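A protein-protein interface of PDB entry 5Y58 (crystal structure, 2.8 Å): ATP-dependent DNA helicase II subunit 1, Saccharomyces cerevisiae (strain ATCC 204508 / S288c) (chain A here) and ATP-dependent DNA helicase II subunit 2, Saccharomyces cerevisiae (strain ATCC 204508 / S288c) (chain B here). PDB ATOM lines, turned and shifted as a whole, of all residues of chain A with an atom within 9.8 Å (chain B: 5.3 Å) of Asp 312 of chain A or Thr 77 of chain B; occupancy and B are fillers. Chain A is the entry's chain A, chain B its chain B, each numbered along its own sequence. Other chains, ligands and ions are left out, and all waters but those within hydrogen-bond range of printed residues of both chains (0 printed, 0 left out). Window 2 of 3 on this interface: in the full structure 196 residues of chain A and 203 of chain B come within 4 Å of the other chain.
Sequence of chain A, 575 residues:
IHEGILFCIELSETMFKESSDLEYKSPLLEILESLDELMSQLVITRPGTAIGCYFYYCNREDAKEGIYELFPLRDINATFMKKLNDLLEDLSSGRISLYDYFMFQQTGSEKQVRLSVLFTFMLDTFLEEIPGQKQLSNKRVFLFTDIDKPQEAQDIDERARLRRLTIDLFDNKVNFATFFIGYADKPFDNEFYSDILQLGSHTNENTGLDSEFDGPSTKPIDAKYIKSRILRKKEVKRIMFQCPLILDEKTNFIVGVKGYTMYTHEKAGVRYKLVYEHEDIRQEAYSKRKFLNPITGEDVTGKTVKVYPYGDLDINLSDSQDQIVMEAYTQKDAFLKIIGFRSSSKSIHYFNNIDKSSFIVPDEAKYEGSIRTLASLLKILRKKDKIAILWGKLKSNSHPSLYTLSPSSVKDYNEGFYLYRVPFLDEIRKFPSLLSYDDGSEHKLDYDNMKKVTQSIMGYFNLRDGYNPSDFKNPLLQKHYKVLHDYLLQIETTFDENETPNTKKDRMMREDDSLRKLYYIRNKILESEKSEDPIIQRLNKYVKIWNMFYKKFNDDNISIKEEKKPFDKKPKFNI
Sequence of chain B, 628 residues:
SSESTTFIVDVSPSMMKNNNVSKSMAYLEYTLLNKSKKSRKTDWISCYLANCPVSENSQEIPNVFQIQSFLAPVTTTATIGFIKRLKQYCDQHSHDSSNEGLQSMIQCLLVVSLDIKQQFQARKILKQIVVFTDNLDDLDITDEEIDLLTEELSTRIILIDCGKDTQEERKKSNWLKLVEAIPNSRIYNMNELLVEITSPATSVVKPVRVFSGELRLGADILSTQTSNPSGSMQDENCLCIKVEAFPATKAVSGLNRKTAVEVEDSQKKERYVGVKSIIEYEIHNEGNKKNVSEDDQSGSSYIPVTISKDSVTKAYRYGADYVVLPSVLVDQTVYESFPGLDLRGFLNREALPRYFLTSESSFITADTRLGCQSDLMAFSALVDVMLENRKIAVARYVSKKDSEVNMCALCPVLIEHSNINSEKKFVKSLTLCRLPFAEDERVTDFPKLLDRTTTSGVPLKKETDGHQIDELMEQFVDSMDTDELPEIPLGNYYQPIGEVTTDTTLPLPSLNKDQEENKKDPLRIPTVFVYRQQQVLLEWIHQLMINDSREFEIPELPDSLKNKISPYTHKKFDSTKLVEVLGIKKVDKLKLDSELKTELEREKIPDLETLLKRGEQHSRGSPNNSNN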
ATOM      1  N   TYR A 308      -7.397  21.867 -17.591  1.00  0.00           N
ATOM      2  CA  TYR A 308      -7.014  23.183 -17.103  1.00  0.00           C
ATOM      3  C   TYR A 308      -6.237  23.049 -15.802  1.00  0.00           C
ATOM      4  O   TYR A 308      -6.783  22.595 -14.797  1.00  0.00           O
ATOM      5  CB  TYR A 308      -8.243  24.072 -16.887  1.00  0.00           C
ATOM      6  CG  TYR A 308      -8.970  24.457 -18.153  1.00  0.00           C
ATOM      7  CD1 TYR A 308      -8.466  25.443 -18.992  1.00  0.00           C
ATOM      8  CD2 TYR A 308     -10.166  23.846 -18.504  1.00  0.00           C
ATOM      9  CE1 TYR A 308      -9.129  25.801 -20.150  1.00  0.00           C
ATOM     10  CE2 TYR A 308     -10.836  24.199 -19.658  1.00  0.00           C
ATOM     11  CZ  TYR A 308     -10.312  25.176 -20.478  1.00  0.00           C
ATOM     12  OH  TYR A 308     -10.974  25.531 -21.630  1.00  0.00           O
ATOM     13  N   PRO A 309      -4.952  23.431 -15.815  1.00  0.00           N
ATOM     14  CA  PRO A 309      -4.190  23.432 -14.564  1.00  0.00           C
ATOM     15  C   PRO A 309      -4.636  24.567 -13.645  1.00  0.00           C
ATOM     16  O   PRO A 309      -4.770  25.705 -14.093  1.00  0.00           O
ATOM     17  CB  PRO A 309      -2.745  23.629 -15.032  1.00  0.00           C
ATOM     18  CG  PRO A 309      -2.868  24.357 -16.321  1.00  0.00           C
ATOM     19  CD  PRO A 309      -4.127  23.842 -16.966  1.00  0.00           C
ATOM     20  N   TYR A 310      -4.879  24.253 -12.378  1.00  0.00           N
ATOM     21  CA  TYR A 310      -5.315  25.256 -11.417  1.00  0.00           C
ATOM     22  C   TYR A 310      -4.616  25.054 -10.079  1.00  0.00           C
ATOM     23  O   TYR A 310      -5.209  24.555  -9.123  1.00  0.00           O
ATOM     24  CB  TYR A 310      -6.831  25.201 -11.238  1.00  0.00           C
ATOM     25  CG  TYR A 310      -7.444  26.533 -10.875  1.00  0.00           C
ATOM     26  CD1 TYR A 310      -7.312  27.055  -9.596  1.00  0.00           C
ATOM     27  CD2 TYR A 310      -8.156  27.270 -11.811  1.00  0.00           C
ATOM     28  CE1 TYR A 310      -7.866  28.272  -9.260  1.00  0.00           C
ATOM     29  CE2 TYR A 310      -8.715  28.485 -11.487  1.00  0.00           C
ATOM     30  CZ  TYR A 310      -8.569  28.984 -10.210  1.00  0.00           C
ATOM     31  OH  TYR A 310      -9.129  30.198  -9.892  1.00  0.00           O
ATOM     32  N   GLY A 311      -3.350  25.448 -10.017  1.00  0.00           N
ATOM     33  CA  GLY A 311      -2.539  25.205  -8.841  1.00  0.00           C
ATOM     34  C   GLY A 311      -2.194  23.733  -8.794  1.00  0.00           C
ATOM     35  O   GLY A 311      -1.863  23.142  -9.822  1.00  0.00           O
ATOM     36  N   ASP A 312      -2.287  23.130  -7.612  1.00  0.00           N
ATOM     37  CA  ASP A 312      -2.026  21.700  -7.473  1.00  0.00           C
ATOM     38  C   ASP A 312      -3.306  20.906  -7.739  1.00  0.00           C
ATOM     39  O   ASP A 312      -3.544  19.862  -7.130  1.00  0.00           O
ATOM     40  CB  ASP A 312      -1.459  21.373  -6.084  1.00  0.00           C
ATOM     41  CG  ASP A 312      -2.398  21.760  -4.958  1.00  0.00           C
ATOM     42  OD1 ASP A 312      -3.358  22.511  -5.220  1.00  0.00           O
ATOM     43  OD2 ASP A 312      -2.169  21.323  -3.810  1.00  0.00           O
ATOM     44  N   LEU A 313      -4.122  21.414  -8.657  1.00  0.00           N
ATOM     45  CA  LEU A 313      -5.357  20.746  -9.044  1.00  0.00           C
ATOM     46  C   LEU A 313      -5.586  20.862 -10.549  1.00  0.00           C
ATOM     47  O   LEU A 313      -5.368  21.920 -11.136  1.00  0.00           O
ATOM     48  CB  LEU A 313      -6.543  21.334  -8.281  1.00  0.00           C
ATOM     49  CG  LEU A 313      -7.892  20.667  -8.551  1.00  0.00           C
ATOM     50  CD1 LEU A 313      -8.053  19.414  -7.697  1.00  0.00           C
ATOM     51  CD2 LEU A 313      -9.042  21.643  -8.330  1.00  0.00           C
ATOM     52  N   ASP A 314      -6.017  19.766 -11.166  1.00  0.00           N
ATOM     53  CA  ASP A 314      -6.338  19.754 -12.590  1.00  0.00           C
ATOM     54  C   ASP A 314      -7.847  19.622 -12.783  1.00  0.00           C
ATOM     55  O   ASP A 314      -8.508  18.868 -12.070  1.00  0.00           O
ATOM     56  CB  ASP A 314      -5.596  18.616 -13.300  1.00  0.00           C
ATOM     57  CG  ASP A 314      -4.084  18.754 -13.200  1.00  0.00           C
ATOM     58  OD1 ASP A 314      -3.581  19.885 -13.371  1.00  0.00           O
ATOM     59  OD2 ASP A 314      -3.402  17.737 -12.938  1.00  0.00           O
ATOM     60  N   ILE A 315      -8.395  20.361 -13.741  1.00  0.00           N
ATOM     61  CA  ILE A 315      -9.834  20.330 -13.976  1.00  0.00           C
ATOM     62  C   ILE A 315     -10.158  19.965 -15.419  1.00  0.00           C
ATOM     63  O   ILE A 315      -9.801  20.695 -16.345  1.00  0.00           O
ATOM     64  CB  ILE A 315     -10.493  21.679 -13.644  1.00  0.00           C
ATOM     65  CG1 ILE A 315     -10.277  22.032 -12.169  1.00  0.00           C
ATOM     66  CG2 ILE A 315     -11.981  21.644 -13.972  1.00  0.00           C
ATOM     67  CD1 ILE A 315     -10.749  23.421 -11.794  1.00  0.00           C
ATOM     68  N   SER B  36      -3.603  30.780  -5.722  1.00  0.00           N
ATOM     69  CA  SER B  36      -3.249  29.367  -5.776  1.00  0.00           C
ATOM     70  C   SER B  36      -2.687  28.974  -7.137  1.00  0.00           C
ATOM     71  O   SER B  36      -1.890  28.041  -7.242  1.00  0.00           O
ATOM     72  CB  SER B  36      -4.466  28.504  -5.447  1.00  0.00           C
ATOM     73  OG  SER B  36      -5.033  28.875  -4.203  1.00  0.00           O
ATOM     74  N   THR B  75      -1.617  27.033  -1.937  1.00  0.00           N
ATOM     75  CA  THR B  75      -2.030  25.999  -2.875  1.00  0.00           C
ATOM     76  C   THR B  75      -3.549  25.935  -2.976  1.00  0.00           C
ATOM     77  O   THR B  75      -4.262  26.424  -2.099  1.00  0.00           O
ATOM     78  CB  THR B  75      -1.485  24.618  -2.468  1.00  0.00           C
ATOM     79  OG1 THR B  75      -2.183  24.144  -1.312  1.00  0.00           O
ATOM     80  CG2 THR B  75       0.002  24.703  -2.158  1.00  0.00           C
ATOM     81  N   THR B  76      -4.036  25.325  -4.051  1.00  0.00           N
ATOM     82  CA  THR B  76      -5.469  25.194  -4.272  1.00  0.00           C
ATOM     83  C   THR B  76      -6.116  24.351  -3.178  1.00  0.00           C
ATOM     84  O   THR B  76      -7.116  24.759  -2.590  1.00  0.00           O
ATOM     85  CB  THR B  76      -5.771  24.572  -5.649  1.00  0.00           C
ATOM     86  OG1 THR B  76      -5.105  25.326  -6.671  1.00  0.00           O
ATOM     87  CG2 THR B  76      -7.266  24.568  -5.919  1.00  0.00           C
ATOM     88  N   THR B  77      -5.532  23.187  -2.899  1.00  0.00           N
ATOM     89  CA  THR B  77      -6.061  22.274  -1.886  1.00  0.00           C
ATOM     90  C   THR B  77      -6.142  22.927  -0.508  1.00  0.00           C
ATOM     91  O   THR B  77      -7.107  22.719   0.229  1.00  0.00           O
ATOM     92  CB  THR B  77      -5.208  20.993  -1.774  1.00  0.00           C
ATOM     93  OG1 THR B  77      -3.873  21.333  -1.375  1.00  0.00           O
ATOM     94  CG2 THR B  77      -5.169  20.257  -3.105  1.00  0.00           C
ATOM     95  N   ALA B  78      -5.128  23.714  -0.163  1.00  0.00           N
ATOM     96  CA  ALA B  78      -5.101  24.398   1.125  1.00  0.00           C
ATOM     97  C   ALA B  78      -6.188  25.464   1.186  1.00  0.00           C
ATOM     98  O   ALA B  78      -6.760  25.723   2.244  1.00  0.00           O
ATOM     99  CB  ALA B  78      -3.736  25.012   1.372  1.00  0.00           C
ATOM    100  N   THR B  79      -6.469  26.076   0.040  1.00  0.00           N
ATOM    101  CA  THR B  79      -7.525  27.075  -0.056  1.00  0.00           C
ATOM    102  C   THR B  79      -8.894  26.422   0.113  1.00  0.00           C
ATOM    103  O   THR B  79      -9.783  26.985   0.750  1.00  0.00           O
ATOM    104  CB  THR B  79      -7.475  27.828  -1.400  1.00  0.00           C
ATOM    105  OG1 THR B  79      -6.211  28.490  -1.531  1.00  0.00           O
ATOM    106  CG2 THR B  79      -8.591  28.861  -1.481  1.00  0.00           C
ATOM    107  N   ILE B  80      -9.058  25.231  -0.458  1.00  0.00           N
ATOM    108  CA  ILE B  80     -10.290  24.469  -0.285  1.00  0.00           C
ATOM    109  C   ILE B  80     -10.534  24.219   1.198  1.00  0.00           C
ATOM    110  O   ILE B  80     -11.656  24.347   1.687  1.00  0.00           O
ATOM    111  CB  ILE B  80     -10.246  23.115  -1.023  1.00  0.00           C
ATOM    112  CG1 ILE B  80      -9.883  23.306  -2.497  1.00  0.00           C
ATOM    113  CG2 ILE B  80     -11.582  22.399  -0.897  1.00  0.00           C
ATOM    114  CD1 ILE B  80     -10.907  24.067  -3.281  1.00  0.00           C
ATOM    115  N   GLY B  81      -9.462  23.879   1.905  1.00  0.00           N
ATOM    116  CA  GLY B  81      -9.527  23.600   3.328  1.00  0.00           C
ATOM    117  C   GLY B  81      -9.916  24.806   4.160  1.00  0.00           C
ATOM    118  O   GLY B  81     -10.819  24.722   4.991  1.00  0.00           O
ATOM    119  N   ARG B 271      -7.657  12.811 -10.814  1.00  0.00           N
ATOM    120  CA  ARG B 271      -6.210  12.933 -10.659  1.00  0.00           C
ATOM    121  C   ARG B 271      -5.483  12.667 -11.976  1.00  0.00           C
ATOM    122  O   ARG B 271      -5.640  11.603 -12.579  1.00  0.00           O
ATOM    123  CB  ARG B 271      -5.711  11.967  -9.581  1.00  0.00           C
ATOM    124  CG  ARG B 271      -4.431  12.405  -8.890  1.00  0.00           C
ATOM    125  CD  ARG B 271      -4.659  13.682  -8.093  1.00  0.00           C
ATOM    126  NE  ARG B 271      -3.567  13.952  -7.160  1.00  0.00           N
ATOM    127  CZ  ARG B 271      -3.555  14.959  -6.292  1.00  0.00           C
ATOM    128  NH1 ARG B 271      -2.518  15.124  -5.482  1.00  0.00           N
ATOM    129  NH2 ARG B 271      -4.579  15.800  -6.230  1.00  0.00           N
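O of Thr 75 of chain B sits at hydrogen-bond distance from OG of Ser 36 of chain B.
The side-chain hydroxyl (OG) of Ser 36 of chain B sits at hydrogen-bond distance from the side-chain hydroxyl (OG1) of Thr 79 of chain B (2.9 Å).
The side-chain hydroxyl of Thr 77 of chain B lies within hydrogen-bond range of the side-chain hydroxyl of Thr 75 of chain B.
The side-chain hydroxyl (OG1) of Thr 75 of chain B is in hydrogen-bond range of the backbone NH (N) of Ala 78 of chain B, at 3.2 Å.
O of Thr 75 of chain B sits at hydrogen-bond distance from OG1 of Thr 79 of chain B (2.9 Å).
Along chain A the printed residues that touch a printed residue of chain B span positions 310 to 312.
Among the printed residues, no Asp or Glu carboxylate lies within 4 Å of a Lys or Arg side-chain nitrogen of the other chain.
Asp 312 of chain A touches three residues of chain B.
Thr 77 of chain B touches one residue of chain A.
Of chain A, only Asp 312 comes within 4 Å of Thr 75 of chain B.
No residue of chain A comes within 4 Å of Ile 80 of chain B.
Printed residues of chain B within 4 Å of Tyr 310 of chain A: Thr 76 (2.6 Å).
Of the printed residues of chain A, Ser 36 of chain B touches Gly 311.
The nearest residue of chain B that does not touch Asp 312 of chain A is Arg 271 of chain B (4.3 Å).
The nearest residue of chain A that does not touch Thr 77 of chain B is Leu 313 of chain A (5.5 Å).
The nearest printed residue of chain B that does not touch Tyr 310 of chain A is Ser 36 of chain B (4.9 Å).
The backbone carbonyl oxygen (O) of Tyr 310 of chain A is in hydrogen-bond range of the side-chain hydroxyl (OG1) of Thr 76 of chain B, 2.6 Å away.
The backbone NH (N) of Thr 76 of chain B sits at hydrogen-bond distance from the side-chain carboxylate (OD1) of Asp 312 of chain A.
The side-chain hydroxyl (OG1) of Thr 77 of chain B sits at hydrogen-bond distance from the side-chain carboxylate (OD2) of Asp 312 of chain A.
Among the printed residues, pairs that only touch across the chains: Gly 311 of chain A with Ser 36 of chain B (3.3 Å), Gly 311 of chain A with Thr 76 of chain B (3.4 Å) and Asp 312 of chain A with Thr 75 of chain B (3.6 Å).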
